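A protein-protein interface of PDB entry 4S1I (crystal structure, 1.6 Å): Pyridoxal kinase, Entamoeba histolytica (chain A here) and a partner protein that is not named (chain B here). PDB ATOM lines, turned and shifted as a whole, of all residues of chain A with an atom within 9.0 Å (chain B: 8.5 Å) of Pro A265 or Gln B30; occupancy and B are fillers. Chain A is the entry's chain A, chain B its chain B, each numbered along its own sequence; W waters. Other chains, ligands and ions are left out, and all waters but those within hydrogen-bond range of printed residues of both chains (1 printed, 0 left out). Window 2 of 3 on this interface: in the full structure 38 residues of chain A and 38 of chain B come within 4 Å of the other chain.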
ATOM      1  N   PHE A  16      11.882  17.254 -28.624  1.00  0.00           N
ATOM      2  CA  PHE A  16      10.816  18.140 -28.253  1.00  0.00           C
ATOM      3  C   PHE A  16       9.537  17.336 -28.287  1.00  0.00           C
ATOM      4  O   PHE A  16       8.924  17.222 -29.363  1.00  0.00           O
ATOM      5  CB  PHE A  16      10.820  19.333 -29.239  1.00  0.00           C
ATOM      6  CG  PHE A  16      12.190  19.965 -29.431  1.00  0.00           C
ATOM      7  CD1 PHE A  16      12.812  20.630 -28.385  1.00  0.00           C
ATOM      8  CD2 PHE A  16      12.832  19.943 -30.658  1.00  0.00           C
ATOM      9  CE1 PHE A  16      14.133  21.161 -28.525  1.00  0.00           C
ATOM     10  CE2 PHE A  16      14.094  20.507 -30.817  1.00  0.00           C
ATOM     11  CZ  PHE A  16      14.756  21.081 -29.754  1.00  0.00           C
ATOM     12  N   ILE A  24       9.376  25.200 -23.696  1.00  0.00           N
ATOM     13  CA  ILE A  24       9.883  26.140 -24.651  1.00  0.00           C
ATOM     14  C   ILE A  24       8.783  27.178 -25.009  1.00  0.00           C
ATOM     15  O   ILE A  24       9.076  28.355 -25.042  1.00  0.00           O
ATOM     16  CB  ILE A  24      10.409  25.466 -25.888  1.00  0.00           C
ATOM     17  CG1 ILE A  24      11.611  24.669 -25.556  1.00  0.00           C
ATOM     18  CG2 ILE A  24      10.882  26.518 -26.886  1.00  0.00           C
ATOM     19  CD1 ILE A  24      11.919  23.461 -26.458  1.00  0.00           C
ATOM     20  N   SER A  28       8.555  31.018 -23.699  1.00  0.00           N
ATOM     21  CA  SER A  28       8.621  32.040 -24.718  1.00  0.00           C
ATOM     22  C   SER A  28       7.455  33.045 -24.689  1.00  0.00           C
ATOM     23  O   SER A  28       7.650  34.217 -24.905  1.00  0.00           O
ATOM     24  CB  SER A  28       8.623  31.422 -26.096  1.00  0.00           C
ATOM     25  OG  SER A  28       8.831  32.568 -26.951  1.00  0.00           O
ATOM     26  N   THR A 244       0.632  29.105 -37.001  1.00  0.00           N
ATOM     27  CA  THR A 244       1.982  29.059 -36.548  1.00  0.00           C
ATOM     28  C   THR A 244       2.625  27.721 -36.855  1.00  0.00           C
ATOM     29  O   THR A 244       3.708  27.675 -37.382  1.00  0.00           O
ATOM     30  CB  THR A 244       2.092  29.423 -35.078  1.00  0.00           C
ATOM     31  OG1 THR A 244       1.736  30.834 -34.957  1.00  0.00           O
ATOM     32  CG2 THR A 244       3.503  29.195 -34.568  1.00  0.00           C
ATOM     33  N   THR A 247       3.421  27.452 -40.450  1.00  0.00           N
ATOM     34  CA  THR A 247       4.634  28.235 -40.690  1.00  0.00           C
ATOM     35  C   THR A 247       5.882  27.504 -40.265  1.00  0.00           C
ATOM     36  O   THR A 247       6.842  27.495 -41.006  1.00  0.00           O
ATOM     37  CB  THR A 247       4.508  29.599 -40.018  1.00  0.00           C
ATOM     38  OG1 THR A 247       3.428  30.289 -40.613  1.00  0.00           O
ATOM     39  CG2 THR A 247       5.804  30.415 -40.152  1.00  0.00           C
ATOM     40  N   ILE A 248       5.845  26.848 -39.100  1.00  0.00           N
ATOM     41  CA  ILE A 248       6.964  26.066 -38.617  1.00  0.00           C
ATOM     42  C   ILE A 248       7.276  24.897 -39.573  1.00  0.00           C
ATOM     43  O   ILE A 248       8.441  24.621 -39.978  1.00  0.00           O
ATOM     44  CB  ILE A 248       6.703  25.549 -37.189  1.00  0.00           C
ATOM     45  CG1 ILE A 248       6.734  26.769 -36.254  1.00  0.00           C
ATOM     46  CG2 ILE A 248       7.726  24.471 -36.845  1.00  0.00           C
ATOM     47  CD1 ILE A 248       6.275  26.411 -34.887  1.00  0.00           C
ATOM     48  N   ASN A 259      12.096  21.834 -35.216  1.00  0.00           N
ATOM     49  CA  ASN A 259      13.030  22.279 -34.208  1.00  0.00           C
ATOM     50  C   ASN A 259      12.425  23.514 -33.602  1.00  0.00           C
ATOM     51  O   ASN A 259      12.527  24.606 -34.113  1.00  0.00           O
ATOM     52  CB  ASN A 259      14.367  22.551 -34.855  1.00  0.00           C
ATOM     53  CG  ASN A 259      15.434  22.733 -33.830  1.00  0.00           C
ATOM     54  OD1 ASN A 259      15.362  23.660 -33.005  1.00  0.00           O
ATOM     55  ND2 ASN A 259      16.382  21.811 -33.798  1.00  0.00           N
ATOM     56  N   ILE A 260      11.829  23.306 -32.462  1.00  0.00           N
ATOM     57  CA  ILE A 260      11.105  24.301 -31.764  1.00  0.00           C
ATOM     58  C   ILE A 260      12.044  25.429 -31.326  1.00  0.00           C
ATOM     59  O   ILE A 260      11.648  26.605 -31.381  1.00  0.00           O
ATOM     60  CB  ILE A 260      10.433  23.655 -30.541  1.00  0.00           C
ATOM     61  CG1 ILE A 260       9.384  22.635 -30.958  1.00  0.00           C
ATOM     62  CG2 ILE A 260       9.631  24.758 -29.772  1.00  0.00           C
ATOM     63  CD1 ILE A 260       8.374  23.210 -31.984  1.00  0.00           C
ATOM     64  N   ILE A 261      13.295  25.083 -30.929  1.00  0.00           N
ATOM     65  CA  ILE A 261      14.294  26.074 -30.539  1.00  0.00           C
ATOM     66  C   ILE A 261      14.565  27.052 -31.683  1.00  0.00           C
ATOM     67  O   ILE A 261      14.594  28.252 -31.540  1.00  0.00           O
ATOM     68  CB  ILE A 261      15.631  25.363 -30.110  1.00  0.00           C
ATOM     69  CG1 ILE A 261      15.374  24.549 -28.827  1.00  0.00           C
ATOM     70  CG2 ILE A 261      16.764  26.332 -29.935  1.00  0.00           C
ATOM     71  CD1 ILE A 261      14.929  25.352 -27.655  1.00  0.00           C
ATOM     72  N   ASN A 262      14.892  26.534 -32.832  1.00  0.00           N
ATOM     73  CA  ASN A 262      15.083  27.397 -33.971  1.00  0.00           C
ATOM     74  C   ASN A 262      13.877  28.236 -34.425  1.00  0.00           C
ATOM     75  O   ASN A 262      14.033  29.198 -35.148  1.00  0.00           O
ATOM     76  CB  ASN A 262      15.557  26.570 -35.091  1.00  0.00           C
ATOM     77  CG  ASN A 262      17.002  26.208 -34.923  1.00  0.00           C
ATOM     78  OD1 ASN A 262      17.438  25.146 -35.350  1.00  0.00           O
ATOM     79  ND2 ASN A 262      17.767  27.113 -34.325  1.00  0.00           N
ATOM     80  N   CYS A 263      12.704  27.799 -34.040  1.00  0.00           N
ATOM     81  CA  CYS A 263      11.486  28.453 -34.515  1.00  0.00           C
ATOM     82  C   CYS A 263      10.892  29.316 -33.339  1.00  0.00           C
ATOM     83  O   CYS A 263       9.807  29.847 -33.488  1.00  0.00           O
ATOM     84  CB  CYS A 263      10.519  27.393 -35.059  1.00  0.00           C
ATOM     85  SG  CYS A 263      10.788  26.869 -36.812  1.00  0.00           S
ATOM     86  N   ILE A 264      11.678  29.577 -32.282  1.00  0.00           N
ATOM     87  CA  ILE A 264      11.174  30.434 -31.155  1.00  0.00           C
ATOM     88  C   ILE A 264      10.585  31.773 -31.674  1.00  0.00           C
ATOM     89  O   ILE A 264       9.478  32.138 -31.268  1.00  0.00           O
ATOM     90  CB  ILE A 264      12.284  30.610 -30.085  1.00  0.00           C
ATOM     91  CG1 ILE A 264      12.262  29.354 -29.211  1.00  0.00           C
ATOM     92  CG2 ILE A 264      12.089  31.901 -29.289  1.00  0.00           C
ATOM     93  CD1 ILE A 264      13.440  29.280 -28.263  1.00  0.00           C
ATOM     94  N   PRO A 265      11.254  32.447 -32.645  1.00  0.00           N
ATOM     95  CA  PRO A 265      10.684  33.750 -33.132  1.00  0.00           C
ATOM     96  C   PRO A 265       9.352  33.646 -33.818  1.00  0.00           C
ATOM     97  O   PRO A 265       8.747  34.685 -34.003  1.00  0.00           O
ATOM     98  CB  PRO A 265      11.706  34.222 -34.160  1.00  0.00           C
ATOM     99  CG  PRO A 265      12.967  33.571 -33.755  1.00  0.00           C
ATOM    100  CD  PRO A 265      12.598  32.247 -33.203  1.00  0.00           C
ATOM    101  N   TYR A 266       8.886  32.449 -34.166  1.00  0.00           N
ATOM    102  CA  TYR A 266       7.591  32.287 -34.798  1.00  0.00           C
ATOM    103  C   TYR A 266       6.473  31.950 -33.808  1.00  0.00           C
ATOM    104  O   TYR A 266       5.297  32.010 -34.184  1.00  0.00           O
ATOM    105  CB  TYR A 266       7.653  31.137 -35.816  1.00  0.00           C
ATOM    106  CG  TYR A 266       8.592  31.265 -37.010  1.00  0.00           C
ATOM    107  CD1 TYR A 266       8.430  32.250 -37.977  1.00  0.00           C
ATOM    108  CD2 TYR A 266       9.604  30.310 -37.190  1.00  0.00           C
ATOM    109  CE1 TYR A 266       9.295  32.319 -39.072  1.00  0.00           C
ATOM    110  CE2 TYR A 266      10.465  30.358 -38.254  1.00  0.00           C
ATOM    111  CZ  TYR A 266      10.318  31.364 -39.200  1.00  0.00           C
ATOM    112  OH  TYR A 266      11.194  31.376 -40.269  1.00  0.00           O
ATOM    113  N   LEU A 267       6.821  31.502 -32.603  1.00  0.00           N
ATOM    114  CA  LEU A 267       5.816  30.932 -31.692  1.00  0.00           C
ATOM    115  C   LEU A 267       4.673  31.892 -31.383  1.00  0.00           C
ATOM    116  O   LEU A 267       3.557  31.414 -31.194  1.00  0.00           O
ATOM    117  CB  LEU A 267       6.451  30.383 -30.408  1.00  0.00           C
ATOM    118  CG  LEU A 267       7.453  29.264 -30.600  1.00  0.00           C
ATOM    119  CD1 LEU A 267       8.237  29.007 -29.293  1.00  0.00           C
ATOM    120  CD2 LEU A 267       6.788  28.015 -31.168  1.00  0.00           C
ATOM    121  N   LYS A 268       4.994  33.154 -31.279  1.00  0.00           N
ATOM    122  CA  LYS A 268       4.008  34.150 -30.830  1.00  0.00           C
ATOM    123  C   LYS A 268       3.404  34.820 -32.041  1.00  0.00           C
ATOM    124  O   LYS A 268       2.847  35.939 -31.979  1.00  0.00           O
ATOM    125  CB  LYS A 268       4.640  35.148 -29.879  1.00  0.00           C
ATOM    126  CG  LYS A 268       5.069  34.562 -28.577  1.00  0.00           C
ATOM    127  CD  LYS A 268       5.570  35.667 -27.651  1.00  0.00           C
ATOM    128  CE  LYS A 268       4.331  36.348 -27.073  1.00  0.00           C
ATOM    129  NZ  LYS A 268       4.460  37.596 -26.182  1.00  0.00           N
ATOM    130  N   GLY A 269       3.468  34.157 -33.199  1.00  0.00           N
ATOM    131  CA  GLY A 269       2.884  34.715 -34.418  1.00  0.00           C
ATOM    132  C   GLY A 269       1.383  34.960 -34.260  1.00  0.00           C
ATOM    133  O   GLY A 269       0.720  34.172 -33.525  1.00  0.00           O
ATOM    134  N   THR A 270       0.888  36.038 -34.827  1.00  0.00           N
ATOM    135  CA  THR A 270      -0.533  36.394 -34.659  1.00  0.00           C
ATOM    136  C   THR A 270      -1.309  36.208 -35.935  1.00  0.00           C
ATOM    137  O   THR A 270      -2.499  36.507 -35.959  1.00  0.00           O
ATOM    138  CB  THR A 270      -0.728  37.839 -34.115  1.00  0.00           C
ATOM    139  OG1 THR A 270      -0.194  38.783 -35.029  1.00  0.00           O
ATOM    140  CG2 THR A 270      -0.090  38.066 -32.791  1.00  0.00           C
ATOM    141  N   MET B   1      20.264  22.122 -36.599  1.00  0.00           N
ATOM    142  CA  MET B   1      21.131  20.936 -36.895  1.00  0.00           C
ATOM    143  C   MET B   1      21.000  19.891 -35.744  1.00  0.00           C
ATOM    144  O   MET B   1      19.968  19.195 -35.543  1.00  0.00           O
ATOM    145  CB  MET B   1      22.632  21.357 -37.084  1.00  0.00           C
ATOM    146  CG  MET B   1      22.998  22.113 -38.342  1.00  0.00           C
ATOM    147  SD  MET B   1      23.167  21.078 -39.807  1.00  0.00           S
ATOM    148  CE  MET B   1      23.783  22.249 -41.048  1.00  0.00           C
ATOM    149  N   THR B   2      22.015  19.902 -34.881  1.00  0.00           N
ATOM    150  CA  THR B   2      22.267  18.825 -33.972  1.00  0.00           C
ATOM    151  C   THR B   2      22.573  19.405 -32.574  1.00  0.00           C
ATOM    152  O   THR B   2      22.742  20.607 -32.392  1.00  0.00           O
ATOM    153  CB  THR B   2      23.482  18.058 -34.413  1.00  0.00           C
ATOM    154  OG1 THR B   2      24.521  19.029 -34.552  1.00  0.00           O
ATOM    155  CG2 THR B   2      23.160  17.370 -35.735  1.00  0.00           C
ATOM    156  N   LYS B   4      24.502  20.660 -29.516  1.00  0.00           N
ATOM    157  CA  LYS B   4      25.835  21.198 -29.322  1.00  0.00           C
ATOM    158  C   LYS B   4      26.341  21.192 -27.918  1.00  0.00           C
ATOM    159  O   LYS B   4      27.531  21.199 -27.604  1.00  0.00           O
ATOM    160  CB  LYS B   4      25.860  22.630 -29.866  1.00  0.00           C
ATOM    161  CG  LYS B   4      27.056  23.507 -29.558  1.00  0.00           C
ATOM    162  CD  LYS B   4      26.928  24.911 -30.201  1.00  0.00           C
ATOM    163  CE  LYS B   4      27.245  24.876 -31.658  1.00  0.00           C
ATOM    164  NZ  LYS B   4      27.419  26.239 -32.173  1.00  0.00           N
ATOM    165  N   VAL B   5      25.391  21.173 -26.967  1.00  0.00           N
ATOM    166  CA  VAL B   5      25.659  21.201 -25.566  1.00  0.00           C
ATOM    167  C   VAL B   5      25.019  20.033 -24.817  1.00  0.00           C
ATOM    168  O   VAL B   5      23.883  19.653 -25.121  1.00  0.00           O
ATOM    169  CB  VAL B   5      25.088  22.471 -24.901  1.00  0.00           C
ATOM    170  CG1 VAL B   5      25.443  22.523 -23.452  1.00  0.00           C
ATOM    171  CG2 VAL B   5      25.580  23.727 -25.582  1.00  0.00           C
ATOM    172  N   MET B  23      17.828  25.516 -19.148  1.00  0.00           N
ATOM    173  CA  MET B  23      16.863  25.380 -20.198  1.00  0.00           C
ATOM    174  C   MET B  23      16.342  26.769 -20.677  1.00  0.00           C
ATOM    175  O   MET B  23      16.338  27.046 -21.887  1.00  0.00           O
ATOM    176  CB  MET B  23      15.675  24.486 -19.859  1.00  0.00           C
ATOM    177  CG  MET B  23      15.970  23.045 -19.536  1.00  0.00           C
ATOM    178  SD  MET B  23      14.596  22.206 -18.606  1.00  0.00           S
ATOM    179  CE  MET B  23      15.457  20.775 -18.012  1.00  0.00           C
ATOM    180  N   ILE B  24      15.948  27.661 -19.787  1.00  0.00           N
ATOM    181  CA  ILE B  24      15.476  28.889 -20.200  1.00  0.00           C
ATOM    182  C   ILE B  24      16.513  29.685 -20.986  1.00  0.00           C
ATOM    183  O   ILE B  24      16.187  30.328 -21.987  1.00  0.00           O
ATOM    184  CB  ILE B  24      14.918  29.707 -18.947  1.00  0.00           C
ATOM    185  CG1 ILE B  24      13.735  28.956 -18.421  1.00  0.00           C
ATOM    186  CG2 ILE B  24      14.442  31.055 -19.444  1.00  0.00           C
ATOM    187  CD1 ILE B  24      13.498  29.243 -16.949  1.00  0.00           C
ATOM    188  N   ILE B  25      17.731  29.713 -20.479  1.00  0.00           N
ATOM    189  CA  ILE B  25      18.760  30.553 -21.021  1.00  0.00           C
ATOM    190  C   ILE B  25      19.230  29.973 -22.376  1.00  0.00           C
ATOM    191  O   ILE B  25      19.257  30.703 -23.361  1.00  0.00           O
ATOM    192  CB  ILE B  25      19.899  30.741 -20.013  1.00  0.00           C
ATOM    193  CG1 ILE B  25      19.332  31.518 -18.796  1.00  0.00           C
ATOM    194  CG2 ILE B  25      21.073  31.450 -20.653  1.00  0.00           C
ATOM    195  CD1 ILE B  25      20.179  31.415 -17.589  1.00  0.00           C
ATOM    196  N   LEU B  26      19.573  28.698 -22.354  1.00  0.00           N
ATOM    197  CA  LEU B  26      20.075  28.115 -23.634  1.00  0.00           C
ATOM    198  C   LEU B  26      18.974  28.092 -24.690  1.00  0.00           C
ATOM    199  O   LEU B  26      19.264  28.292 -25.847  1.00  0.00           O
ATOM    200  CB  LEU B  26      20.629  26.721 -23.461  1.00  0.00           C
ATOM    201  CG  LEU B  26      21.927  26.692 -22.599  1.00  0.00           C
ATOM    202  CD1 LEU B  26      22.244  25.296 -22.098  1.00  0.00           C
ATOM    203  CD2 LEU B  26      23.047  27.305 -23.412  1.00  0.00           C
ATOM    204  N   ASP B  27      17.723  27.822 -24.309  1.00  0.00           N
ATOM    205  CA  ASP B  27      16.637  27.852 -25.260  1.00  0.00           C
ATOM    206  C   ASP B  27      16.503  29.304 -25.837  1.00  0.00           C
ATOM    207  O   ASP B  27      16.407  29.573 -27.061  1.00  0.00           O
ATOM    208  CB  ASP B  27      15.286  27.460 -24.662  1.00  0.00           C
ATOM    209  CG  ASP B  27      15.132  26.021 -24.227  1.00  0.00           C
ATOM    210  OD1 ASP B  27      15.994  25.119 -24.594  1.00  0.00           O
ATOM    211  OD2 ASP B  27      14.136  25.733 -23.449  1.00  0.00           O
ATOM    212  N   SER B  28      16.604  30.349 -25.013  1.00  0.00           N
ATOM    213  CA  SER B  28      16.474  31.754 -25.453  1.00  0.00           C
ATOM    214  C   SER B  28      17.607  32.185 -26.376  1.00  0.00           C
ATOM    215  O   SER B  28      17.341  32.857 -27.351  1.00  0.00           O
ATOM    216  CB  SER B  28      16.482  32.687 -24.262  1.00  0.00           C
ATOM    217  OG  SER B  28      16.222  33.943 -24.857  1.00  0.00           O
ATOM    218  N   PHE B  29      18.825  31.656 -26.090  1.00  0.00           N
ATOM    219  CA  PHE B  29      19.956  31.846 -26.981  1.00  0.00           C
ATOM    220  C   PHE B  29      19.908  30.927 -28.191  1.00  0.00           C
ATOM    221  O   PHE B  29      20.811  31.052 -29.083  1.00  0.00           O
ATOM    222  CB  PHE B  29      21.260  31.646 -26.242  1.00  0.00           C
ATOM    223  CG  PHE B  29      21.773  32.851 -25.489  1.00  0.00           C
ATOM    224  CD1 PHE B  29      21.473  33.067 -24.161  1.00  0.00           C
ATOM    225  CD2 PHE B  29      22.680  33.719 -26.097  1.00  0.00           C
ATOM    226  CE1 PHE B  29      22.055  34.114 -23.481  1.00  0.00           C
ATOM    227  CE2 PHE B  29      23.286  34.749 -25.432  1.00  0.00           C
ATOM    228  CZ  PHE B  29      22.927  34.970 -24.117  1.00  0.00           C
ATOM    229  N   GLN B  30      18.920  30.096 -28.320  1.00  0.00           N
ATOM    230  CA  GLN B  30      18.701  29.187 -29.446  1.00  0.00           C
ATOM    231  C   GLN B  30      19.942  28.232 -29.662  1.00  0.00           C
ATOM    232  O   GLN B  30      20.342  27.956 -30.808  1.00  0.00           O
ATOM    233  CB  GLN B  30      18.335  29.875 -30.701  1.00  0.00           C
ATOM    234  CG  GLN B  30      16.965  30.552 -30.534  1.00  0.00           C
ATOM    235  CD  GLN B  30      16.615  31.347 -31.781  1.00  0.00           C
ATOM    236  OE1 GLN B  30      17.207  32.424 -32.046  1.00  0.00           O
ATOM    237  NE2 GLN B  30      15.780  30.801 -32.622  1.00  0.00           N
ATOM    238  N   ILE B  31      20.465  27.764 -28.567  1.00  0.00           N
ATOM    239  CA  ILE B  31      21.566  26.845 -28.532  1.00  0.00           C
ATOM    240  C   ILE B  31      20.976  25.463 -28.264  1.00  0.00           C
ATOM    241  O   ILE B  31      20.429  25.199 -27.213  1.00  0.00           O
ATOM    242  CB  ILE B  31      22.605  27.230 -27.499  1.00  0.00           C
ATOM    243  CG1 ILE B  31      23.255  28.569 -27.851  1.00  0.00           C
ATOM    244  CG2 ILE B  31      23.733  26.144 -27.332  1.00  0.00           C
ATOM    245  CD1 ILE B  31      24.074  29.206 -26.769  1.00  0.00           C
ATOM    246  N   GLN B  32      21.186  24.566 -29.256  1.00  0.00           N
ATOM    247  CA  GLN B  32      20.570  23.238 -29.152  1.00  0.00           C
ATOM    248  C   GLN B  32      21.345  22.360 -28.098  1.00  0.00           C
ATOM    249  O   GLN B  32      22.597  22.175 -28.203  1.00  0.00           O
ATOM    250  CB  GLN B  32      20.622  22.506 -30.473  1.00  0.00           C
ATOM    251  CG  GLN B  32      19.640  21.342 -30.252  1.00  0.00           C
ATOM    252  CD  GLN B  32      18.902  20.924 -31.447  1.00  0.00           C
ATOM    253  OE1 GLN B  32      18.407  21.773 -32.168  1.00  0.00           O
ATOM    254  NE2 GLN B  32      18.815  19.596 -31.668  1.00  0.00           N
ATOM    255  N   SER B  33      20.598  21.883 -27.109  1.00  0.00           N
ATOM    256  CA  SER B  33      21.193  21.313 -25.926  1.00  0.00           C
ATOM    257  C   SER B  33      20.443  20.113 -25.396  1.00  0.00           C
ATOM    258  O   SER B  33      19.211  20.018 -25.605  1.00  0.00           O
ATOM    259  CB  SER B  33      21.244  22.363 -24.818  1.00  0.00           C
ATOM    260  OG  SER B  33      21.841  23.537 -25.212  1.00  0.00           O
ATOM    261  N   SER B 226      26.719  30.603 -22.821  1.00  0.00           N
ATOM    262  CA  SER B 226      26.062  30.982 -24.073  1.00  0.00           C
ATOM    263  C   SER B 226      26.926  31.900 -24.871  1.00  0.00           C
ATOM    264  O   SER B 226      27.146  31.744 -26.096  1.00  0.00           O
ATOM    265  CB  SER B 226      24.716  31.593 -23.795  1.00  0.00           C
ATOM    266  OG  SER B 226      23.822  30.616 -23.308  1.00  0.00           O
ATOM    267  N   ILE B 229      29.915  30.093 -26.310  1.00  0.00           N
ATOM    268  CA  ILE B 229      29.440  29.368 -27.473  1.00  0.00           C
ATOM    269  C   ILE B 229      29.276  30.196 -28.687  1.00  0.00           C
ATOM    270  O   ILE B 229      29.623  29.744 -29.842  1.00  0.00           O
ATOM    271  CB  ILE B 229      28.183  28.550 -27.102  1.00  0.00           C
ATOM    272  CG1 ILE B 229      28.480  27.464 -26.039  1.00  0.00           C
ATOM    273  CG2 ILE B 229      27.460  27.977 -28.343  1.00  0.00           C
ATOM    274  CD1 ILE B 229      27.231  26.719 -25.585  1.00  0.00           C
ATOM    275  N   LYS B 230      28.764  31.430 -28.539  1.00  0.00           N
ATOM    276  CA  LYS B 230      28.604  32.358 -29.634  1.00  0.00           C
ATOM    277  C   LYS B 230      29.963  32.969 -30.127  1.00  0.00           C
ATOM    278  O   LYS B 230      29.988  33.780 -31.061  1.00  0.00           O
ATOM    279  CB  LYS B 230      27.671  33.471 -29.245  1.00  0.00           C
ATOM    280  CG  LYS B 230      26.252  33.016 -28.928  1.00  0.00           C
ATOM    281  CD  LYS B 230      25.445  32.404 -30.027  1.00  0.00           C
ATOM    282  CE  LYS B 230      23.972  32.216 -29.607  1.00  0.00           C
ATOM    283  NZ  LYS B 230      23.212  31.453 -30.622  1.00  0.00           N
ATOM    284  N   LYS B 268      19.949  38.072 -23.407  1.00  0.00           N
ATOM    285  CA  LYS B 268      20.908  38.188 -24.541  1.00  0.00           C
ATOM    286  C   LYS B 268      21.495  39.587 -24.598  1.00  0.00           C
ATOM    287  O   LYS B 268      21.962  40.117 -25.676  1.00  0.00           O
ATOM    288  CB  LYS B 268      20.225  37.820 -25.854  1.00  0.00           C
ATOM    289  CG  LYS B 268      19.859  36.383 -25.946  1.00  0.00           C
ATOM    290  CD  LYS B 268      19.331  36.078 -27.341  1.00  0.00           C
ATOM    291  CE  LYS B 268      20.572  35.972 -28.263  1.00  0.00           C
ATOM    292  NZ  LYS B 268      20.397  35.746 -29.715  1.00  0.00           N
HETATM  293  O   HOH W   1      19.841  26.348 -32.879  1.00  0.00           O
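Water W1 lies within hydrogen-bond range of ND2 of Asn A262 (2.6 Å) and O of Gln B30 (2.7 Å).
The side-chain amide oxygen (OE1) of Gln B32 lies within hydrogen-bond range of the side-chain amide nitrogen (ND2) of Asn A259 (2.6 Å). NE2 of Gln B30 sits at hydrogen-bond distance from O of Ile A261, 3.0 Å away. The side-chain amide nitrogen of Gln B30 lies within hydrogen-bond range of the backbone carbonyl oxygen of Asn A262 (3.5 Å).
Ile A24 touches Asp B27 (CG1 to OD2, 3.5 Å). CD1 of Ile A261 touches OD1 of Asp B27 (3.2 Å). Ile A264 touches Asp B27. CD of Pro A265 touches NE2 of Gln B30, 3.5 Å away.
N of Asn A262 lies within hydrogen-bond range of OD1 of Asn A259. OD1 of Asn A259 lies close to N of Ile A261 (3.3 Å). The backbone NH (N) of Val B5 is in hydrogen-bond range of the backbone carbonyl oxygen (O) of Gln B32, at 3.2 Å. O of Gln B32 is in hydrogen-bond range of N of Lys B4 (2.8 Å).
Of the 19 printed residues of chain B, 3 touch a printed residue of chain A. Printed residues of chain A that touch a printed residue of chain B: Ile A24, Asn A259, Ile A261, Asn A262, Ile A264 and Pro A265. Hydrophobic or aromatic side chains of chain A that line the printed part of chain B: Ile A24, Ile A261, Ile A264 and Pro A265. Among the printed residues, 7 pairs touch across the chains. Among the printed residues, no Asp or Glu carboxylate lies within 4 Å of a Lys or Arg side-chain nitrogen of the other chain.
Of the printed residues of chain B, Ile A24 touches Asp B27 (3.5 Å). Of the printed residues of chain B, Asn A259 touches Gln B32. Printed residues of chain B within 4 Å of Asn A262: Gln B30 (3.5 Å). Printed residues of chain B within 4 Å of Ile A264: Asp B27. Printed residues of chain B within 4 Å of Pro A265: Gln B30. Printed residues of chain A within 4 Å of Asp B27: Ile A24, Ile A261 and Ile A264. Gln B30 touches just these residues of chain A: Ile A261, Asn A262 and Pro A265. The nearest residue of chain A that does not touch Gln B30 is Ile A264 (4.3 Å).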
